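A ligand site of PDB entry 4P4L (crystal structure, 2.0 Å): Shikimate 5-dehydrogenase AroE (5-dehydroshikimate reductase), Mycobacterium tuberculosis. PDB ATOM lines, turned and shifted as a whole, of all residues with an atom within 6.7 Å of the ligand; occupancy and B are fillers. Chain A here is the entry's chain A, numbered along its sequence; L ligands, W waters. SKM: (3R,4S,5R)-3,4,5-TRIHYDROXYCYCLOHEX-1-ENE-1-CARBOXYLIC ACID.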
ATOM      1  N   VAL A  10       0.773  -1.253  -9.219  1.00  0.00           N
ATOM      2  CA  VAL A  10       1.881  -0.662  -8.471  1.00  0.00           C
ATOM      3  C   VAL A  10       3.095  -0.405  -9.398  1.00  0.00           C
ATOM      4  O   VAL A  10       3.477  -1.287 -10.159  1.00  0.00           O
ATOM      5  CB  VAL A  10       2.269  -1.556  -7.270  1.00  0.00           C
ATOM      6  CG1 VAL A  10       2.643  -2.999  -7.716  1.00  0.00           C
ATOM      7  CG2 VAL A  10       3.405  -0.900  -6.461  1.00  0.00           C
ATOM      8  N   ILE A  15       9.976  -4.663  -9.098  1.00  0.00           N
ATOM      9  CA  ILE A  15       8.576  -4.682  -8.686  1.00  0.00           C
ATOM     10  C   ILE A  15       8.039  -6.104  -8.511  1.00  0.00           C
ATOM     11  O   ILE A  15       6.952  -6.296  -7.956  1.00  0.00           O
ATOM     12  CB  ILE A  15       7.701  -3.868  -9.650  1.00  0.00           C
ATOM     13  CG1 ILE A  15       6.367  -3.505  -8.998  1.00  0.00           C
ATOM     14  CG2 ILE A  15       7.507  -4.593 -10.970  1.00  0.00           C
ATOM     15  CD1 ILE A  15       6.514  -2.548  -7.835  1.00  0.00           C
ATOM     16  N   HIS A  17       8.454  -8.588  -6.596  1.00  0.00           N
ATOM     17  CA  HIS A  17       8.124  -9.154  -5.285  1.00  0.00           C
ATOM     18  C   HIS A  17       7.112  -8.342  -4.480  1.00  0.00           C
ATOM     19  O   HIS A  17       6.871  -8.640  -3.302  1.00  0.00           O
ATOM     20  CB  HIS A  17       9.405  -9.392  -4.475  1.00  0.00           C
ATOM     21  CG  HIS A  17      10.263 -10.499  -5.012  1.00  0.00           C
ATOM     22  ND1 HIS A  17      11.617 -10.559  -4.794  1.00  0.00           N
ATOM     23  CD2 HIS A  17       9.946 -11.590  -5.757  1.00  0.00           C
ATOM     24  CE1 HIS A  17      12.115 -11.637  -5.377  1.00  0.00           C
ATOM     25  NE2 HIS A  17      11.113 -12.282  -5.963  1.00  0.00           N
ATOM     26  N   SER A  18       6.520  -7.317  -5.114  1.00  0.00           N
ATOM     27  CA  SER A  18       5.473  -6.520  -4.479  1.00  0.00           C
ATOM     28  C   SER A  18       4.320  -7.408  -4.024  1.00  0.00           C
ATOM     29  O   SER A  18       3.854  -8.267  -4.773  1.00  0.00           O
ATOM     30  CB  SER A  18       4.895  -5.483  -5.449  1.00  0.00           C
ATOM     31  OG  SER A  18       3.877  -4.739  -4.801  1.00  0.00           O
ATOM     32  N   ARG A  19       3.858  -7.186  -2.787  1.00  0.00           N
ATOM     33  CA  ARG A  19       2.711  -7.921  -2.290  1.00  0.00           C
ATOM     34  C   ARG A  19       1.499  -7.005  -2.314  1.00  0.00           C
ATOM     35  O   ARG A  19       0.439  -7.347  -1.785  1.00  0.00           O
ATOM     36  CB  ARG A  19       2.965  -8.415  -0.868  1.00  0.00           C
ATOM     37  CG  ARG A  19       4.373  -9.008  -0.645  1.00  0.00           C
ATOM     38  CD  ARG A  19       4.584 -10.349  -1.350  1.00  0.00           C
ATOM     39  NE  ARG A  19       5.430 -11.272  -0.581  1.00  0.00           N
ATOM     40  CZ  ARG A  19       6.771 -11.271  -0.575  1.00  0.00           C
ATOM     41  NH1 ARG A  19       7.453 -10.380  -1.284  1.00  0.00           N
ATOM     42  NH2 ARG A  19       7.430 -12.156   0.154  1.00  0.00           N
ATOM     43  N   SER A  20       1.647  -5.831  -2.924  1.00  0.00           N
ATOM     44  CA  SER A  20       0.510  -4.945  -3.136  1.00  0.00           C
ATOM     45  C   SER A  20      -0.686  -5.591  -3.862  1.00  0.00           C
ATOM     46  O   SER A  20      -1.817  -5.424  -3.412  1.00  0.00           O
ATOM     47  CB  SER A  20       0.930  -3.652  -3.851  1.00  0.00           C
ATOM     48  OG  SER A  20       1.417  -2.709  -2.921  1.00  0.00           O
ATOM     49  N   PRO A  21      -0.436  -6.304  -4.980  1.00  0.00           N
ATOM     50  CA  PRO A  21      -1.559  -6.934  -5.692  1.00  0.00           C
ATOM     51  C   PRO A  21      -2.404  -7.838  -4.790  1.00  0.00           C
ATOM     52  O   PRO A  21      -3.620  -7.762  -4.841  1.00  0.00           O
ATOM     53  CB  PRO A  21      -0.873  -7.776  -6.761  1.00  0.00           C
ATOM     54  CG  PRO A  21       0.393  -6.988  -7.082  1.00  0.00           C
ATOM     55  CD  PRO A  21       0.828  -6.475  -5.722  1.00  0.00           C
ATOM     56  N   HIS A  24      -4.572  -5.469  -2.559  1.00  0.00           N
ATOM     57  CA  HIS A  24      -5.580  -4.703  -3.286  1.00  0.00           C
ATOM     58  C   HIS A  24      -6.673  -5.573  -3.885  1.00  0.00           C
ATOM     59  O   HIS A  24      -7.860  -5.273  -3.752  1.00  0.00           O
ATOM     60  CB  HIS A  24      -4.909  -3.852  -4.374  1.00  0.00           C
ATOM     61  CG  HIS A  24      -4.311  -2.565  -3.861  1.00  0.00           C
ATOM     62  ND1 HIS A  24      -4.960  -1.355  -3.970  1.00  0.00           N
ATOM     63  CD2 HIS A  24      -3.147  -2.316  -3.216  1.00  0.00           C
ATOM     64  CE1 HIS A  24      -4.205  -0.407  -3.412  1.00  0.00           C
ATOM     65  NE2 HIS A  24      -3.111  -0.975  -2.950  1.00  0.00           N
ATOM     66  N   TYR A  38      -5.256  -5.239 -10.881  1.00  0.00           N
ATOM     67  CA  TYR A  38      -4.156  -4.533 -10.206  1.00  0.00           C
ATOM     68  C   TYR A  38      -2.885  -5.227 -10.670  1.00  0.00           C
ATOM     69  O   TYR A  38      -2.712  -6.427 -10.433  1.00  0.00           O
ATOM     70  CB  TYR A  38      -4.292  -4.652  -8.681  1.00  0.00           C
ATOM     71  CG  TYR A  38      -3.342  -3.772  -7.883  1.00  0.00           C
ATOM     72  CD1 TYR A  38      -2.018  -4.158  -7.658  1.00  0.00           C
ATOM     73  CD2 TYR A  38      -3.768  -2.568  -7.358  1.00  0.00           C
ATOM     74  CE1 TYR A  38      -1.156  -3.348  -6.914  1.00  0.00           C
ATOM     75  CE2 TYR A  38      -2.911  -1.751  -6.624  1.00  0.00           C
ATOM     76  CZ  TYR A  38      -1.608  -2.162  -6.406  1.00  0.00           C
ATOM     77  OH  TYR A  38      -0.762  -1.355  -5.647  1.00  0.00           O
ATOM     78  N   SER A  63      -0.374   2.805  -7.107  1.00  0.00           N
ATOM     79  CA  SER A  63       0.599   2.835  -6.029  1.00  0.00           C
ATOM     80  C   SER A  63       1.985   3.043  -6.626  1.00  0.00           C
ATOM     81  O   SER A  63       2.270   2.595  -7.750  1.00  0.00           O
ATOM     82  CB  SER A  63       0.564   1.535  -5.237  1.00  0.00           C
ATOM     83  OG  SER A  63      -0.766   1.237  -4.815  1.00  0.00           O
ATOM     84  N   VAL A  64       2.849   3.753  -5.898  1.00  0.00           N
ATOM     85  CA  VAL A  64       4.193   4.012  -6.410  1.00  0.00           C
ATOM     86  C   VAL A  64       5.171   3.646  -5.328  1.00  0.00           C
ATOM     87  O   VAL A  64       5.089   4.167  -4.204  1.00  0.00           O
ATOM     88  CB  VAL A  64       4.405   5.486  -6.781  1.00  0.00           C
ATOM     89  CG1 VAL A  64       5.866   5.711  -7.282  1.00  0.00           C
ATOM     90  CG2 VAL A  64       3.410   5.909  -7.825  1.00  0.00           C
ATOM     91  N   THR A  65       6.093   2.745  -5.628  1.00  0.00           N
ATOM     92  CA  THR A  65       7.096   2.404  -4.652  1.00  0.00           C
ATOM     93  C   THR A  65       8.456   2.892  -5.159  1.00  0.00           C
ATOM     94  O   THR A  65       8.507   3.643  -6.153  1.00  0.00           O
ATOM     95  CB  THR A  65       7.074   0.901  -4.283  1.00  0.00           C
ATOM     96  OG1 THR A  65       7.975   0.668  -3.179  1.00  0.00           O
ATOM     97  CG2 THR A  65       7.484   0.037  -5.464  1.00  0.00           C
ATOM     98  N   MET A  66       9.544   2.510  -4.487  1.00  0.00           N
ATOM     99  CA  MET A  66      10.892   2.942  -4.906  1.00  0.00           C
ATOM    100  C   MET A  66      11.105   2.536  -6.367  1.00  0.00           C
ATOM    101  O   MET A  66      10.692   1.451  -6.779  1.00  0.00           O
ATOM    102  CB  MET A  66      11.972   2.278  -4.039  1.00  0.00           C
ATOM    103  CG  MET A  66      11.986   2.761  -2.578  1.00  0.00           C
ATOM    104  SD  MET A  66      10.523   2.270  -1.631  1.00  0.00           S
ATOM    105  CE  MET A  66      10.373   3.639  -0.449  1.00  0.00           C
ATOM    106  N   LYS A  69       8.877   7.696  -5.987  1.00  0.00           N
ATOM    107  CA  LYS A  69       7.981   8.508  -5.146  1.00  0.00           C
ATOM    108  C   LYS A  69       8.187  10.017  -5.273  1.00  0.00           C
ATOM    109  O   LYS A  69       7.256  10.811  -5.054  1.00  0.00           O
ATOM    110  CB  LYS A  69       8.066   8.066  -3.669  1.00  0.00           C
ATOM    111  CG  LYS A  69       7.710   6.588  -3.464  1.00  0.00           C
ATOM    112  CD  LYS A  69       7.536   6.280  -1.961  1.00  0.00           C
ATOM    113  CE  LYS A  69       7.152   4.832  -1.768  1.00  0.00           C
ATOM    114  NZ  LYS A  69       7.279   4.386  -0.333  1.00  0.00           N
ATOM    115  N   ALA A  89       5.531  10.942  -2.683  1.00  0.00           N
ATOM    116  CA  ALA A  89       4.190  10.353  -2.810  1.00  0.00           C
ATOM    117  C   ALA A  89       4.237   8.893  -3.239  1.00  0.00           C
ATOM    118  O   ALA A  89       4.900   8.548  -4.222  1.00  0.00           O
ATOM    119  CB  ALA A  89       3.360  11.147  -3.810  1.00  0.00           C
ATOM    120  N   ASN A  90       3.504   8.045  -2.511  1.00  0.00           N
ATOM    121  CA  ASN A  90       3.422   6.644  -2.900  1.00  0.00           C
ATOM    122  C   ASN A  90       2.075   6.353  -3.569  1.00  0.00           C
ATOM    123  O   ASN A  90       1.759   5.195  -3.866  1.00  0.00           O
ATOM    124  CB  ASN A  90       3.603   5.751  -1.681  1.00  0.00           C
ATOM    125  CG  ASN A  90       2.393   5.779  -0.776  1.00  0.00           C
ATOM    126  OD1 ASN A  90       1.679   6.788  -0.716  1.00  0.00           O
ATOM    127  ND2 ASN A  90       2.109   4.656  -0.110  1.00  0.00           N
ATOM    128  N   THR A  91       1.293   7.401  -3.822  1.00  0.00           N
ATOM    129  CA  THR A  91      -0.073   7.236  -4.298  1.00  0.00           C
ATOM    130  C   THR A  91      -0.451   8.314  -5.317  1.00  0.00           C
ATOM    131  O   THR A  91      -0.370   9.501  -5.014  1.00  0.00           O
ATOM    132  CB  THR A  91      -1.082   7.327  -3.111  1.00  0.00           C
ATOM    133  OG1 THR A  91      -0.664   6.447  -2.064  1.00  0.00           O
ATOM    134  CG2 THR A  91      -2.501   6.936  -3.573  1.00  0.00           C
ATOM    135  N   ASN A 103       0.655  10.666   0.253  1.00  0.00           N
ATOM    136  CA  ASN A 103       1.614   9.731   0.799  1.00  0.00           C
ATOM    137  C   ASN A 103       0.968   8.960   1.941  1.00  0.00           C
ATOM    138  O   ASN A 103       0.727   9.522   3.003  1.00  0.00           O
ATOM    139  CB  ASN A 103       2.900  10.436   1.250  1.00  0.00           C
ATOM    140  CG  ASN A 103       3.999   9.450   1.626  1.00  0.00           C
ATOM    141  OD1 ASN A 103       3.772   8.553   2.453  1.00  0.00           O
ATOM    142  ND2 ASN A 103       5.176   9.587   1.005  1.00  0.00           N
ATOM    143  N   THR A 104       0.692   7.675   1.702  1.00  0.00           N
ATOM    144  CA  THR A 104       0.035   6.839   2.709  1.00  0.00           C
ATOM    145  C   THR A 104       1.034   6.079   3.585  1.00  0.00           C
ATOM    146  O   THR A 104       0.628   5.355   4.512  1.00  0.00           O
ATOM    147  CB  THR A 104      -0.975   5.854   2.053  1.00  0.00           C
ATOM    148  OG1 THR A 104      -0.272   4.843   1.305  1.00  0.00           O
ATOM    149  CG2 THR A 104      -1.924   6.636   1.150  1.00  0.00           C
ATOM    150  N   ASP A 105       2.320   6.231   3.305  1.00  0.00           N
ATOM    151  CA  ASP A 105       3.336   5.577   4.127  1.00  0.00           C
ATOM    152  C   ASP A 105       3.245   6.105   5.549  1.00  0.00           C
ATOM    153  O   ASP A 105       3.626   5.416   6.507  1.00  0.00           O
ATOM    154  CB  ASP A 105       4.773   5.799   3.580  1.00  0.00           C
ATOM    155  CG  ASP A 105       5.054   4.992   2.332  1.00  0.00           C
ATOM    156  OD1 ASP A 105       4.636   3.797   2.255  1.00  0.00           O
ATOM    157  OD2 ASP A 105       5.704   5.538   1.402  1.00  0.00           O
ATOM    158  N   THR A 128      11.442   5.799   3.664  1.00  0.00           N
ATOM    159  CA  THR A 128      10.217   6.095   4.393  1.00  0.00           C
ATOM    160  C   THR A 128      10.487   6.779   5.740  1.00  0.00           C
ATOM    161  O   THR A 128       9.559   6.966   6.525  1.00  0.00           O
ATOM    162  CB  THR A 128       9.353   4.849   4.582  1.00  0.00           C
ATOM    163  OG1 THR A 128      10.063   3.893   5.385  1.00  0.00           O
ATOM    164  CG2 THR A 128       9.040   4.235   3.222  1.00  0.00           C
ATOM    165  N   TYR A 215      10.547  -6.465   4.903  1.00  0.00           N
ATOM    166  CA  TYR A 215       9.681  -7.645   5.037  1.00  0.00           C
ATOM    167  C   TYR A 215      10.136  -8.900   4.283  1.00  0.00           C
ATOM    168  O   TYR A 215       9.592  -9.995   4.517  1.00  0.00           O
ATOM    169  CB  TYR A 215       8.202  -7.295   4.779  1.00  0.00           C
ATOM    170  CG  TYR A 215       7.795  -6.937   3.354  1.00  0.00           C
ATOM    171  CD1 TYR A 215       7.586  -7.920   2.408  1.00  0.00           C
ATOM    172  CD2 TYR A 215       7.547  -5.620   2.993  1.00  0.00           C
ATOM    173  CE1 TYR A 215       7.176  -7.599   1.118  1.00  0.00           C
ATOM    174  CE2 TYR A 215       7.127  -5.290   1.713  1.00  0.00           C
ATOM    175  CZ  TYR A 215       6.948  -6.277   0.779  1.00  0.00           C
ATOM    176  OH  TYR A 215       6.537  -5.951  -0.499  1.00  0.00           O
ATOM    177  N   LEU A 240       2.996  -2.343   5.078  1.00  0.00           N
ATOM    178  CA  LEU A 240       2.377  -2.452   3.769  1.00  0.00           C
ATOM    179  C   LEU A 240       0.868  -2.517   3.921  1.00  0.00           C
ATOM    180  O   LEU A 240       0.127  -1.913   3.126  1.00  0.00           O
ATOM    181  CB  LEU A 240       2.895  -3.687   3.026  1.00  0.00           C
ATOM    182  CG  LEU A 240       2.486  -3.761   1.565  1.00  0.00           C
ATOM    183  CD1 LEU A 240       3.344  -2.806   0.713  1.00  0.00           C
ATOM    184  CD2 LEU A 240       2.587  -5.199   1.041  1.00  0.00           C
ATOM    185  N   GLN A 243      -0.542   1.124   4.957  1.00  0.00           N
ATOM    186  CA  GLN A 243      -0.486   2.145   3.900  1.00  0.00           C
ATOM    187  C   GLN A 243      -1.478   1.830   2.768  1.00  0.00           C
ATOM    188  O   GLN A 243      -1.949   2.725   2.076  1.00  0.00           O
ATOM    189  CB  GLN A 243       0.947   2.339   3.363  1.00  0.00           C
ATOM    190  CG  GLN A 243       1.554   1.110   2.684  1.00  0.00           C
ATOM    191  CD  GLN A 243       1.131   0.993   1.245  1.00  0.00           C
ATOM    192  OE1 GLN A 243       1.131   1.973   0.495  1.00  0.00           O
ATOM    193  NE2 GLN A 243       0.760  -0.240   0.838  1.00  0.00           N
ATOM    194  N   ALA A 244      -1.817   0.551   2.621  1.00  0.00           N
ATOM    195  CA  ALA A 244      -2.702   0.151   1.534  1.00  0.00           C
ATOM    196  C   ALA A 244      -4.152   0.548   1.781  1.00  0.00           C
ATOM    197  O   ALA A 244      -4.917   0.759   0.829  1.00  0.00           O
ATOM    198  CB  ALA A 244      -2.585  -1.365   1.274  1.00  0.00           C
ATOM    199  N   GLN A 247      -4.997   3.816   0.291  1.00  0.00           N
ATOM    200  CA  GLN A 247      -4.957   3.687  -1.178  1.00  0.00           C
ATOM    201  C   GLN A 247      -6.240   3.047  -1.706  1.00  0.00           C
ATOM    202  O   GLN A 247      -6.790   3.475  -2.712  1.00  0.00           O
ATOM    203  CB  GLN A 247      -3.723   2.912  -1.644  1.00  0.00           C
ATOM    204  CG  GLN A 247      -2.380   3.619  -1.341  1.00  0.00           C
ATOM    205  CD  GLN A 247      -1.207   2.922  -2.021  1.00  0.00           C
ATOM    206  OE1 GLN A 247      -1.269   1.721  -2.333  1.00  0.00           O
ATOM    207  NE2 GLN A 247      -0.111   3.658  -2.249  1.00  0.00           N
HETATM  208  O12 SKM L   1       4.448   2.905  -0.309  1.00  0.00           O
HETATM  209  C8  SKM L   1       4.313   1.500  -0.572  1.00  0.00           C
HETATM  210  C6  SKM L   1       5.666   0.866  -0.389  1.00  0.00           C
HETATM  211  O7  SKM L   1       6.654   1.661  -1.008  1.00  0.00           O
HETATM  212  C5  SKM L   1       5.674  -0.418  -1.028  1.00  0.00           C
HETATM  213  C4  SKM L   1       4.737  -0.915  -1.840  1.00  0.00           C
HETATM  214  C1  SKM L   1       4.934  -2.297  -2.418  1.00  0.00           C
HETATM  215  O2  SKM L   1       4.108  -2.737  -3.252  1.00  0.00           O
HETATM  216  O3  SKM L   1       5.945  -2.971  -2.057  1.00  0.00           O
HETATM  217  C10 SKM L   1       3.459  -0.136  -2.247  1.00  0.00           C
HETATM  218  C9  SKM L   1       3.744   1.365  -1.951  1.00  0.00           C
HETATM  219  O11 SKM L   1       2.502   1.982  -2.061  1.00  0.00           O
HETATM  220  O   HOH W   1       8.361  -2.027  -2.841  1.00  0.00           O
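Water W1 bridges O3 of the ligand (2.7 Å) and OG1 of Thr 65 (2.7 Å).
The side-chain amide nitrogen of Gln 243 sits at hydrogen-bond distance from the backbone carbonyl oxygen of Leu 240, 2.9 Å away.
The side-chain amide oxygen (OE1) of Gln 247 lies within hydrogen-bond range of a ring nitrogen (NE2) of His 24 (3.3 Å).
OG1 of Thr 91 is in hydrogen-bond range of OD1 of Asn 90, at 2.7 Å.
N of Val 64 lies within hydrogen-bond range of O of Asn 90.
OD2 of Asp 105 lies within salt-bridge range of NZ of Lys 69 (2.6 Å).
OE1 of Gln 243 lies within hydrogen-bond range of ND2 of Asn 90, at 2.9 Å.
The backbone carbonyl oxygen (O) of Asn 90 is in hydrogen-bond range of the side-chain amide nitrogen (NE2) of Gln 247 (2.9 Å).
The side-chain amide oxygen of Asn 90 lies within hydrogen-bond range of the backbone NH of Thr 104 (2.8 Å).
Val 10 touches the ligand (CG2 to O2, 3.8 Å).
Ser 63 touches the ligand (CB to O11, 3.7 Å).
Val 64 touches the ligand (O to C9, 3.8 Å).
Met 66 touches the ligand.
Leu 240 touches the ligand (CD1 to C4, 3.5 Å).
Hydrophobic or aromatic side chains that line the ligand: Val 10, Met 66 and Leu 240.
The nearest printed residue that does not touch the ligand is Arg 19 (4.5 Å).
OE1 of Gln 243 sits at hydrogen-bond distance from O11 of the ligand.
An oxygen (O2) of the ligand is in hydrogen-bond range of the side-chain hydroxyl (OG) of Ser 18 (2.5 Å).
An oxygen (O12) of the ligand is in hydrogen-bond range of the side-chain amide nitrogen of Asn 90, 2.9 Å away.
The side-chain hydroxyl (OG1) of Thr 65 is in hydrogen-bond range of an oxygen (O7) of the ligand, at 2.7 Å.
OH of Tyr 215 lies within hydrogen-bond range of O3 of the ligand.
The side-chain carboxylate (OD1) of Asp 105 lies within hydrogen-bond range of an oxygen (O12) of the ligand (2.7 Å).
An oxygen (O2) of the ligand lies within hydrogen-bond range of the side-chain hydroxyl of Ser 20, at 2.7 Å.
An oxygen (O7) of the ligand sits at hydrogen-bond distance from the side-chain amino group of Lys 69.
NE2 of Gln 247 lies within hydrogen-bond range of O11 of the ligand.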
